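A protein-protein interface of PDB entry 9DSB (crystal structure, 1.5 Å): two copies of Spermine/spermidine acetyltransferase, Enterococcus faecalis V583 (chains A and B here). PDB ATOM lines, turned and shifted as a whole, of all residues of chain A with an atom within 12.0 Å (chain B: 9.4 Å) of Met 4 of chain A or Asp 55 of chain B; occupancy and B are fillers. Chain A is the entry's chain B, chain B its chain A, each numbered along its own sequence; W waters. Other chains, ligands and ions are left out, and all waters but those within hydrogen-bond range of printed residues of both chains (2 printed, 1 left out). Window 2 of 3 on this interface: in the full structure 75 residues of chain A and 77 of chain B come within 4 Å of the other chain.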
ATOM      1  N   ALA A   3       3.397  17.483  32.297  1.00  0.00           N
ATOM      2  CA  ALA A   3       3.456  18.678  33.176  1.00  0.00           C
ATOM      3  C   ALA A   3       2.932  19.895  32.418  1.00  0.00           C
ATOM      4  O   ALA A   3       3.199  20.043  31.225  1.00  0.00           O
ATOM      5  CB  ALA A   3       4.873  18.899  33.664  1.00  0.00           C
ATOM      6  N   MET A   4       2.172  20.747  33.117  1.00  0.00           N
ATOM      7  CA  MET A   4       1.697  22.002  32.560  1.00  0.00           C
ATOM      8  C   MET A   4       2.491  23.139  33.203  1.00  0.00           C
ATOM      9  O   MET A   4       2.560  23.226  34.431  1.00  0.00           O
ATOM     10  CB  MET A   4       0.189  22.171  32.796  1.00  0.00           C
ATOM     11  CG  MET A   4      -0.520  22.967  31.709  1.00  0.00           C
ATOM     12  SD  MET A   4      -2.283  23.244  31.990  1.00  0.00           S
ATOM     13  CE  MET A   4      -2.240  24.063  33.590  1.00  0.00           C
ATOM     14  N   GLU A   5       3.124  23.968  32.360  1.00  0.00           N
ATOM     15  CA  GLU A   5       4.033  25.013  32.808  1.00  0.00           C
ATOM     16  C   GLU A   5       3.682  26.330  32.120  1.00  0.00           C
ATOM     17  O   GLU A   5       4.404  26.774  31.236  1.00  0.00           O
ATOM     18  CB  GLU A   5       5.486  24.653  32.490  1.00  0.00           C
ATOM     19  CG  GLU A   5       5.993  23.405  33.205  1.00  0.00           C
ATOM     20  CD  GLU A   5       7.339  22.911  32.698  1.00  0.00           C
ATOM     21  OE1 GLU A   5       8.033  23.667  31.985  1.00  0.00           O
ATOM     22  OE2 GLU A   5       7.675  21.746  32.984  1.00  0.00           O
ATOM     23  N   ILE A   6       2.588  26.961  32.565  1.00  0.00           N
ATOM     24  CA  ILE A   6       2.063  28.151  31.916  1.00  0.00           C
ATOM     25  C   ILE A   6       2.836  29.376  32.394  1.00  0.00           C
ATOM     26  O   ILE A   6       3.013  29.567  33.594  1.00  0.00           O
ATOM     27  CB  ILE A   6       0.559  28.315  32.199  1.00  0.00           C
ATOM     28  CG1 ILE A   6      -0.224  27.030  31.926  1.00  0.00           C
ATOM     29  CG2 ILE A   6      -0.009  29.513  31.438  1.00  0.00           C
ATOM     30  CD1 ILE A   6      -0.287  26.620  30.470  1.00  0.00           C
ATOM     31  N   HIS A   7       3.270  30.210  31.443  1.00  0.00           N
ATOM     32  CA  HIS A   7       3.899  31.482  31.764  1.00  0.00           C
ATOM     33  C   HIS A   7       3.671  32.462  30.616  1.00  0.00           C
ATOM     34  O   HIS A   7       3.220  32.070  29.544  1.00  0.00           O
ATOM     35  CB  HIS A   7       5.379  31.284  32.119  1.00  0.00           C
ATOM     36  CG  HIS A   7       6.214  30.739  31.017  1.00  0.00           C
ATOM     37  ND1 HIS A   7       7.042  31.552  30.276  1.00  0.00           N
ATOM     38  CD2 HIS A   7       6.351  29.507  30.516  1.00  0.00           C
ATOM     39  CE1 HIS A   7       7.671  30.819  29.369  1.00  0.00           C
ATOM     40  NE2 HIS A   7       7.268  29.575  29.497  1.00  0.00           N
ATOM     41  N   PHE A   8       3.984  33.735  30.877  1.00  0.00           N
ATOM     42  CA  PHE A   8       3.705  34.828  29.960  1.00  0.00           C
ATOM     43  C   PHE A   8       5.003  35.556  29.639  1.00  0.00           C
ATOM     44  O   PHE A   8       5.778  35.861  30.543  1.00  0.00           O
ATOM     45  CB  PHE A   8       2.718  35.808  30.593  1.00  0.00           C
ATOM     46  CG  PHE A   8       1.378  35.165  30.908  1.00  0.00           C
ATOM     47  CD1 PHE A   8       1.180  34.478  32.103  1.00  0.00           C
ATOM     48  CD2 PHE A   8       0.340  35.206  29.987  1.00  0.00           C
ATOM     49  CE1 PHE A   8      -0.032  33.867  32.373  1.00  0.00           C
ATOM     50  CE2 PHE A   8      -0.876  34.603  30.270  1.00  0.00           C
ATOM     51  CZ  PHE A   8      -1.055  33.933  31.456  1.00  0.00           C
ATOM     52  N   GLU A   9       5.213  35.847  28.349  1.00  0.00           N
ATOM     53  CA  GLU A   9       6.379  36.594  27.909  1.00  0.00           C
ATOM     54  C   GLU A   9       5.920  37.828  27.146  1.00  0.00           C
ATOM     55  O   GLU A   9       4.990  37.749  26.349  1.00  0.00           O
ATOM     56  CB  GLU A   9       7.308  35.770  27.018  1.00  0.00           C
ATOM     57  CG  GLU A   9       7.849  34.522  27.707  1.00  0.00           C
ATOM     58  CD  GLU A   9       8.841  33.745  26.867  1.00  0.00           C
ATOM     59  OE1 GLU A   9       9.153  34.206  25.750  1.00  0.00           O
ATOM     60  OE2 GLU A   9       9.307  32.685  27.340  1.00  0.00           O
ATOM     61  N   ASN A  15      10.098  36.633  19.698  1.00  0.00           N
ATOM     62  CA  ASN A  15       8.933  35.770  19.563  1.00  0.00           C
ATOM     63  C   ASN A  15       7.771  36.408  18.794  1.00  0.00           C
ATOM     64  O   ASN A  15       6.728  35.776  18.654  1.00  0.00           O
ATOM     65  CB  ASN A  15       8.454  35.277  20.925  1.00  0.00           C
ATOM     66  CG  ASN A  15       8.068  36.401  21.861  1.00  0.00           C
ATOM     67  OD1 ASN A  15       8.053  37.574  21.470  1.00  0.00           O
ATOM     68  ND2 ASN A  15       7.764  36.067  23.107  1.00  0.00           N
ATOM     69  N   ALA A  18       6.452  34.405  15.961  1.00  0.00           N
ATOM     70  CA  ALA A  18       5.778  33.223  16.477  1.00  0.00           C
ATOM     71  C   ALA A  18       4.333  33.562  16.849  1.00  0.00           C
ATOM     72  O   ALA A  18       3.413  32.824  16.503  1.00  0.00           O
ATOM     73  CB  ALA A  18       6.531  32.660  17.662  1.00  0.00           C
ATOM     74  N   VAL A  19       4.146  34.689  17.551  1.00  0.00           N
ATOM     75  CA  VAL A  19       2.823  35.163  17.938  1.00  0.00           C
ATOM     76  C   VAL A  19       2.012  35.517  16.688  1.00  0.00           C
ATOM     77  O   VAL A  19       0.836  35.180  16.597  1.00  0.00           O
ATOM     78  CB  VAL A  19       2.925  36.349  18.919  1.00  0.00           C
ATOM     79  CG1 VAL A  19       1.572  37.021  19.154  1.00  0.00           C
ATOM     80  CG2 VAL A  19       3.552  35.927  20.245  1.00  0.00           C
ATOM     81  N   LEU A  22       0.358  32.454  15.226  1.00  0.00           N
ATOM     82  CA  LEU A  22      -0.545  31.636  16.030  1.00  0.00           C
ATOM     83  C   LEU A  22      -1.644  31.068  15.131  1.00  0.00           C
ATOM     84  O   LEU A  22      -2.203  31.789  14.302  1.00  0.00           O
ATOM     85  CB  LEU A  22      -1.107  32.437  17.203  1.00  0.00           C
ATOM     86  CG  LEU A  22      -0.240  32.466  18.467  1.00  0.00           C
ATOM     87  CD1 LEU A  22      -0.487  33.714  19.287  1.00  0.00           C
ATOM     88  CD2 LEU A  22      -0.495  31.239  19.318  1.00  0.00           C
ATOM     89  N   GLY B  52       2.816  36.827  24.838  1.00  0.00           N
ATOM     90  CA  GLY B  52       2.697  35.453  24.386  1.00  0.00           C
ATOM     91  C   GLY B  52       2.425  34.531  25.571  1.00  0.00           C
ATOM     92  O   GLY B  52       2.988  34.721  26.651  1.00  0.00           O
ATOM     93  N   ILE B  53       1.538  33.552  25.359  1.00  0.00           N
ATOM     94  CA  ILE B  53       1.208  32.554  26.364  1.00  0.00           C
ATOM     95  C   ILE B  53       1.967  31.278  26.025  1.00  0.00           C
ATOM     96  O   ILE B  53       1.876  30.779  24.903  1.00  0.00           O
ATOM     97  CB  ILE B  53      -0.308  32.291  26.426  1.00  0.00           C
ATOM     98  CG1 ILE B  53      -1.106  33.584  26.604  1.00  0.00           C
ATOM     99  CG2 ILE B  53      -0.620  31.267  27.516  1.00  0.00           C
ATOM    100  CD1 ILE B  53      -2.611  33.388  26.593  1.00  0.00           C
ATOM    101  N   TYR B  54       2.700  30.752  27.011  1.00  0.00           N
ATOM    102  CA  TYR B  54       3.563  29.602  26.807  1.00  0.00           C
ATOM    103  C   TYR B  54       3.176  28.451  27.728  1.00  0.00           C
ATOM    104  O   TYR B  54       2.743  28.666  28.858  1.00  0.00           O
ATOM    105  CB  TYR B  54       5.017  30.001  27.067  1.00  0.00           C
ATOM    106  CG  TYR B  54       5.605  30.874  25.971  1.00  0.00           C
ATOM    107  CD1 TYR B  54       5.424  32.252  25.973  1.00  0.00           C
ATOM    108  CD2 TYR B  54       6.339  30.314  24.931  1.00  0.00           C
ATOM    109  CE1 TYR B  54       5.939  33.047  24.964  1.00  0.00           C
ATOM    110  CE2 TYR B  54       6.864  31.101  23.921  1.00  0.00           C
ATOM    111  CZ  TYR B  54       6.669  32.471  23.940  1.00  0.00           C
ATOM    112  OH  TYR B  54       7.191  33.254  22.954  1.00  0.00           O
ATOM    113  N   ASP B  55       3.333  27.228  27.207  1.00  0.00           N
ATOM    114  CA  ASP B  55       3.456  26.036  28.025  1.00  0.00           C
ATOM    115  C   ASP B  55       4.885  25.537  27.847  1.00  0.00           C
ATOM    116  O   ASP B  55       5.212  24.950  26.815  1.00  0.00           O
ATOM    117  CB  ASP B  55       2.437  24.967  27.660  1.00  0.00           C
ATOM    118  CG  ASP B  55       2.508  23.708  28.513  1.00  0.00           C
ATOM    119  OD1 ASP B  55       3.128  23.765  29.597  1.00  0.00           O
ATOM    120  OD2 ASP B  55       1.959  22.672  28.083  1.00  0.00           O
ATOM    121  N   GLY B  56       5.732  25.808  28.847  1.00  0.00           N
ATOM    122  CA  GLY B  56       7.162  25.596  28.718  1.00  0.00           C
ATOM    123  C   GLY B  56       7.738  26.458  27.597  1.00  0.00           C
ATOM    124  O   GLY B  56       7.637  27.682  27.644  1.00  0.00           O
ATOM    125  N   ASN B  57       8.308  25.808  26.575  1.00  0.00           N
ATOM    126  CA  ASN B  57       8.914  26.515  25.454  1.00  0.00           C
ATOM    127  C   ASN B  57       7.941  26.650  24.284  1.00  0.00           C
ATOM    128  O   ASN B  57       8.273  27.284  23.283  1.00  0.00           O
ATOM    129  CB  ASN B  57      10.201  25.843  24.988  1.00  0.00           C
ATOM    130  CG  ASN B  57      11.315  26.013  25.991  1.00  0.00           C
ATOM    131  OD1 ASN B  57      11.425  27.075  26.615  1.00  0.00           O
ATOM    132  ND2 ASN B  57      12.132  24.986  26.169  1.00  0.00           N
ATOM    133  N   GLN B  58       6.741  26.068  24.412  1.00  0.00           N
ATOM    134  CA  GLN B  58       5.769  26.080  23.330  1.00  0.00           C
ATOM    135  C   GLN B  58       4.828  27.270  23.496  1.00  0.00           C
ATOM    136  O   GLN B  58       4.118  27.368  24.497  1.00  0.00           O
ATOM    137  CB  GLN B  58       4.989  24.766  23.307  1.00  0.00           C
ATOM    138  CG  GLN B  58       3.933  24.667  22.210  1.00  0.00           C
ATOM    139  CD  GLN B  58       4.498  24.806  20.812  1.00  0.00           C
ATOM    140  OE1 GLN B  58       5.473  24.144  20.441  1.00  0.00           O
ATOM    141  NE2 GLN B  58       3.889  25.675  20.016  1.00  0.00           N
ATOM    142  N   LEU B  59       4.816  28.161  22.497  1.00  0.00           N
ATOM    143  CA  LEU B  59       3.825  29.222  22.433  1.00  0.00           C
ATOM    144  C   LEU B  59       2.466  28.594  22.135  1.00  0.00           C
ATOM    145  O   LEU B  59       2.302  27.968  21.085  1.00  0.00           O
ATOM    146  CB  LEU B  59       4.196  30.246  21.361  1.00  0.00           C
ATOM    147  CG  LEU B  59       3.218  31.416  21.196  1.00  0.00           C
ATOM    148  CD1 LEU B  59       3.339  32.392  22.353  1.00  0.00           C
ATOM    149  CD2 LEU B  59       3.429  32.125  19.872  1.00  0.00           C
ATOM    150  N   ILE B  60       1.498  28.790  23.044  1.00  0.00           N
ATOM    151  CA  ILE B  60       0.178  28.194  22.901  1.00  0.00           C
ATOM    152  C   ILE B  60      -0.904  29.250  22.682  1.00  0.00           C
ATOM    153  O   ILE B  60      -2.048  28.893  22.419  1.00  0.00           O
ATOM    154  CB  ILE B  60      -0.183  27.331  24.121  1.00  0.00           C
ATOM    155  CG1 ILE B  60      -0.201  28.148  25.418  1.00  0.00           C
ATOM    156  CG2 ILE B  60       0.739  26.116  24.208  1.00  0.00           C
ATOM    157  CD1 ILE B  60      -0.923  27.470  26.572  1.00  0.00           C
ATOM    158  N   GLY B  61      -0.576  30.536  22.842  1.00  0.00           N
ATOM    159  CA  GLY B  61      -1.598  31.557  22.718  1.00  0.00           C
ATOM    160  C   GLY B  61      -1.051  32.971  22.869  1.00  0.00           C
ATOM    161  O   GLY B  61       0.153  33.208  22.777  1.00  0.00           O
ATOM    162  N   ILE B  80      -6.183  31.201  22.333  1.00  0.00           N
ATOM    163  CA  ILE B  80      -5.404  29.978  22.423  1.00  0.00           C
ATOM    164  C   ILE B  80      -5.319  29.367  21.028  1.00  0.00           C
ATOM    165  O   ILE B  80      -6.325  29.264  20.330  1.00  0.00           O
ATOM    166  CB  ILE B  80      -6.029  29.009  23.443  1.00  0.00           C
ATOM    167  CG1 ILE B  80      -6.048  29.612  24.852  1.00  0.00           C
ATOM    168  CG2 ILE B  80      -5.331  27.649  23.409  1.00  0.00           C
ATOM    169  CD1 ILE B  80      -4.675  29.928  25.423  1.00  0.00           C
ATOM    170  N   PHE B  84      -4.002  23.504  20.423  1.00  0.00           N
ATOM    171  CA  PHE B  84      -3.897  23.270  21.856  1.00  0.00           C
ATOM    172  C   PHE B  84      -5.229  23.466  22.583  1.00  0.00           C
ATOM    173  O   PHE B  84      -5.253  23.459  23.811  1.00  0.00           O
ATOM    174  CB  PHE B  84      -2.832  24.224  22.405  1.00  0.00           C
ATOM    175  CG  PHE B  84      -1.444  24.059  21.802  1.00  0.00           C
ATOM    176  CD1 PHE B  84      -0.610  23.014  22.194  1.00  0.00           C
ATOM    177  CD2 PHE B  84      -0.967  24.964  20.861  1.00  0.00           C
ATOM    178  CE1 PHE B  84       0.652  22.873  21.640  1.00  0.00           C
ATOM    179  CE2 PHE B  84       0.297  24.818  20.314  1.00  0.00           C
ATOM    180  CZ  PHE B  84       1.105  23.777  20.707  1.00  0.00           C
ATOM    181  N   GLN B  87      -8.108  21.416  25.981  1.00  0.00           N
ATOM    182  CA  GLN B  87      -7.177  20.694  26.836  1.00  0.00           C
ATOM    183  C   GLN B  87      -6.778  21.533  28.053  1.00  0.00           C
ATOM    184  O   GLN B  87      -5.707  21.329  28.620  1.00  0.00           O
ATOM    185  CB  GLN B  87      -5.975  20.276  25.988  1.00  0.00           C
ATOM    186  CG  GLN B  87      -6.290  19.185  24.968  1.00  0.00           C
ATOM    187  CD  GLN B  87      -5.455  19.289  23.709  1.00  0.00           C
ATOM    188  OE1 GLN B  87      -4.222  19.230  23.748  1.00  0.00           O
ATOM    189  NE2 GLN B  87      -6.123  19.453  22.575  1.00  0.00           N
ATOM    190  N   GLY B  88      -7.649  22.466  28.457  1.00  0.00           N
ATOM    191  CA  GLY B  88      -7.544  23.127  29.749  1.00  0.00           C
ATOM    192  C   GLY B  88      -6.568  24.304  29.767  1.00  0.00           C
ATOM    193  O   GLY B  88      -6.316  24.865  30.831  1.00  0.00           O
ATOM    194  N   TYR B  89      -6.036  24.698  28.603  1.00  0.00           N
ATOM    195  CA  TYR B  89      -5.046  25.764  28.549  1.00  0.00           C
ATOM    196  C   TYR B  89      -5.706  27.122  28.777  1.00  0.00           C
ATOM    197  O   TYR B  89      -5.212  27.918  29.571  1.00  0.00           O
ATOM    198  CB  TYR B  89      -4.292  25.807  27.219  1.00  0.00           C
ATOM    199  CG  TYR B  89      -3.100  24.867  27.093  1.00  0.00           C
ATOM    200  CD1 TYR B  89      -2.268  24.578  28.171  1.00  0.00           C
ATOM    201  CD2 TYR B  89      -2.790  24.297  25.868  1.00  0.00           C
ATOM    202  CE1 TYR B  89      -1.179  23.734  28.033  1.00  0.00           C
ATOM    203  CE2 TYR B  89      -1.705  23.450  25.715  1.00  0.00           C
ATOM    204  CZ  TYR B  89      -0.897  23.170  26.800  1.00  0.00           C
ATOM    205  OH  TYR B  89       0.164  22.336  26.619  1.00  0.00           O
ATOM    206  N   GLY B  90      -6.799  27.390  28.054  1.00  0.00           N
ATOM    207  CA  GLY B  90      -7.502  28.659  28.159  1.00  0.00           C
ATOM    208  C   GLY B  90      -7.783  29.034  29.613  1.00  0.00           C
ATOM    209  O   GLY B  90      -7.417  30.115  30.062  1.00  0.00           O
ATOM    210  N   LYS B  91      -8.415  28.117  30.352  1.00  0.00           N
ATOM    211  CA  LYS B  91      -8.832  28.388  31.718  1.00  0.00           C
ATOM    212  C   LYS B  91      -7.601  28.570  32.605  1.00  0.00           C
ATOM    213  O   LYS B  91      -7.538  29.497  33.408  1.00  0.00           O
ATOM    214  CB  LYS B  91      -9.748  27.259  32.198  1.00  0.00           C
ATOM    215  CG  LYS B  91     -10.617  27.586  33.401  1.00  0.00           C
ATOM    216  CD  LYS B  91     -11.331  26.372  33.989  1.00  0.00           C
ATOM    217  CE  LYS B  91     -12.167  25.613  33.001  1.00  0.00           C
ATOM    218  NZ  LYS B  91     -12.750  24.414  33.609  1.00  0.00           N
ATOM    219  N   ALA B  92      -6.608  27.690  32.440  1.00  0.00           N
ATOM    220  CA  ALA B  92      -5.391  27.757  33.237  1.00  0.00           C
ATOM    221  C   ALA B  92      -4.663  29.077  32.990  1.00  0.00           C
ATOM    222  O   ALA B  92      -4.305  29.772  33.937  1.00  0.00           O
ATOM    223  CB  ALA B  92      -4.508  26.568  32.936  1.00  0.00           C
ATOM    224  N   ALA B  93      -4.465  29.418  31.710  1.00  0.00           N
ATOM    225  CA  ALA B  93      -3.820  30.663  31.318  1.00  0.00           C
ATOM    226  C   ALA B  93      -4.645  31.883  31.739  1.00  0.00           C
ATOM    227  O   ALA B  93      -4.087  32.873  32.200  1.00  0.00           O
ATOM    228  CB  ALA B  93      -3.565  30.659  29.825  1.00  0.00           C
ATOM    229  N   CYS B  94      -5.972  31.828  31.583  1.00  0.00           N
ATOM    230  CA  CYS B  94      -6.805  32.966  31.938  1.00  0.00           C
ATOM    231  C   CYS B  94      -6.729  33.245  33.442  1.00  0.00           C
ATOM    232  O   CYS B  94      -6.613  34.396  33.858  1.00  0.00           O
ATOM    233  CB  CYS B  94      -8.248  32.759  31.496  1.00  0.00           C
ATOM    234  SG  CYS B  94      -9.207  34.292  31.512  1.00  0.00           S
ATOM    235  N   ARG B  95      -6.783  32.192  34.263  1.00  0.00           N
ATOM    236  CA  ARG B  95      -6.723  32.370  35.706  1.00  0.00           C
ATOM    237  C   ARG B  95      -5.407  33.045  36.092  1.00  0.00           C
ATOM    238  O   ARG B  95      -5.391  34.013  36.847  1.00  0.00           O
ATOM    239  CB  ARG B  95      -6.869  31.034  36.439  1.00  0.00           C
ATOM    240  CG  ARG B  95      -7.394  31.169  37.863  1.00  0.00           C
ATOM    241  CD  ARG B  95      -7.082  29.951  38.720  1.00  0.00           C
ATOM    242  NE  ARG B  95      -6.905  28.740  37.911  1.00  0.00           N
ATOM    243  CZ  ARG B  95      -7.847  27.862  37.574  1.00  0.00           C
ATOM    244  NH1 ARG B  95      -9.079  27.966  38.044  1.00  0.00           N
ATOM    245  NH2 ARG B  95      -7.543  26.870  36.753  1.00  0.00           N
ATOM    246  N   LEU B  96      -4.298  32.535  35.554  1.00  0.00           N
ATOM    247  CA  LEU B  96      -2.984  33.050  35.910  1.00  0.00           C
ATOM    248  C   LEU B  96      -2.867  34.509  35.478  1.00  0.00           C
ATOM    249  O   LEU B  96      -2.392  35.344  36.244  1.00  0.00           O
ATOM    250  CB  LEU B  96      -1.881  32.165  35.331  1.00  0.00           C
ATOM    251  CG  LEU B  96      -1.854  30.726  35.860  1.00  0.00           C
ATOM    252  CD1 LEU B  96      -0.720  29.930  35.242  1.00  0.00           C
ATOM    253  CD2 LEU B  96      -1.758  30.690  37.380  1.00  0.00           C
HETATM  254  O   HOH W   1       1.132  20.643  29.532  1.00  0.00           O
HETATM  255  O   HOH W   2      10.323  29.447  28.276  1.00  0.00           O
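Printed residues of chain B that touch a printed residue of chain A: Gly 52, Ile 53, Tyr 54, Asp 55, Gly 56, Leu 59, Ile 60, Gly 61, Tyr 89, Ala 92, Ala 93 and Leu 96. Hydrophobic or aromatic side chains of chain B within 4 Å of the printed part of chain A: Ile 53, Tyr 54, Leu 59, Tyr 89, Ala 92 and Leu 96. Hydrophobic or aromatic side chains of chain A that line the printed part of chain B: Met 4, Ile 6, His 7, Phe 8, Ala 18, Val 19 and Leu 22. Among the printed residues, 26 pairs touch across the chains. Among the printed residues, no Asp or Glu carboxylate lies within 4 Å of a Lys or Arg side-chain nitrogen of the other chain.
No residue of chain B comes within 4 Å of Ala 3 of chain A. Met 4 of chain A touches three residues of chain B. Of the printed residues of chain B, Leu 22 of chain A touches Leu 59, Ile 60 and Gly 61. Of the printed residues of chain A, Ile 53 of chain B touches His 7 and Phe 8. Of the printed residues of chain A, Tyr 54 of chain B touches Glu 5 (3.5 Å), Ile 6 (3.2 Å), His 7 (2.9 Å), Glu 9 (3.5 Å) and Asn 15 (2.9 Å). Asp 55 of chain B touches just these residues of chain A: Met 4 and Glu 5. Of the printed residues of chain A, Gly 56 of chain B touches Glu 5 (2.9 Å) and His 7 (2.7 Å). No residue of chain A comes within 4 Å of Gln 58 of chain B. Of chain A, only Leu 22 comes within 4 Å of Ile 60 of chain B. No residue of chain A comes within 4 Å of Gly 88 of chain B. Of chain A, only Met 4 comes within 4 Å of Ala 92 of chain B. The nearest residue of chain A that does not touch Asp 55 of chain B is Ala 3 of chain A (4.1 Å).
No position is printed for both chains. Of the 26 pairs that touch across the chains among the printed residues, none has its exchanged pair printed and touching as well.
Among the printed residues, pairs that only touch across the chains: Met 4 of chain A with Asp 55 of chain B, Met 4 of chain A with Tyr 89 of chain B, Met 4 of chain A with Ala 92 of chain B, Ile 6 of chain A with Tyr 54 of chain B, Ile 6 of chain A with Tyr 89 of chain B, Ile 6 of chain A with Ala 93 of chain B, Ile 6 of chain A with Leu 96 of chain B, His 7 of chain A with Gly 52 of chain B, His 7 of chain A with Ile 53 of chain B, Phe 8 of chain A with Gly 52 of chain B, Phe 8 of chain A with Ile 53 of chain B, Phe 8 of chain A with Ala 93 of chain B, Phe 8 of chain A with Leu 96 of chain B, Glu 9 of chain A with Tyr 54 of chain B, Ala 18 of chain A with Leu 59 of chain B, Val 19 of chain A with Leu 59 of chain B, Leu 22 of chain A with Leu 59 of chain B, Leu 22 of chain A with Ile 60 of chain B and Leu 22 of chain A with Gly 61 of chain B.
The backbone carbonyl oxygen (O) of Glu 9 of chain A is in hydrogen-bond range of the backbone NH (N) of Gly 52 of chain B. The backbone carbonyl oxygen (O) of His 7 of chain A sits at hydrogen-bond distance from the backbone NH (N) of Tyr 54 of chain B (2.9 Å). The side-chain hydroxyl of Tyr 54 of chain B is in hydrogen-bond range of the side-chain amide nitrogen of Asn 15 of chain A, 2.9 Å away. The side-chain carboxylate (OD1) of Asp 55 of chain B sits at hydrogen-bond distance from the backbone NH (N) of Glu 5 of chain A. O of Glu 5 of chain A lies within hydrogen-bond range of N of Gly 56 of chain B (2.9 Å). A ring nitrogen (NE2) of His 7 of chain A is in hydrogen-bond range of the backbone carbonyl oxygen of Gly 56 of chain B, 2.7 Å away. The backbone carbonyl oxygen of Glu 5 of chain A lies close to the backbone carbonyl oxygen of Tyr 54 of chain B, 3.5 Å away.
The backbone carbonyl oxygen of Ile 53 of chain B sits at hydrogen-bond distance from the backbone NH of Ile 60 of chain B, 2.7 Å away. The backbone carbonyl oxygen (O) of Gly 61 of chain B lies within hydrogen-bond range of the backbone NH (N) of Ile 53 of chain B, 3.0 Å away.
Water W1 bridges OD2 of Asp 55 of chain B (2.6 Å) and O of Ala 3 of chain A (2.7 Å). Water W2 lies within hydrogen-bond range of OD1 of Asn 57 of chain B (3.1 Å), O of Gly 56 of chain B (3.3 Å) and NE2 of His 7 of chain A (3.3 Å).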
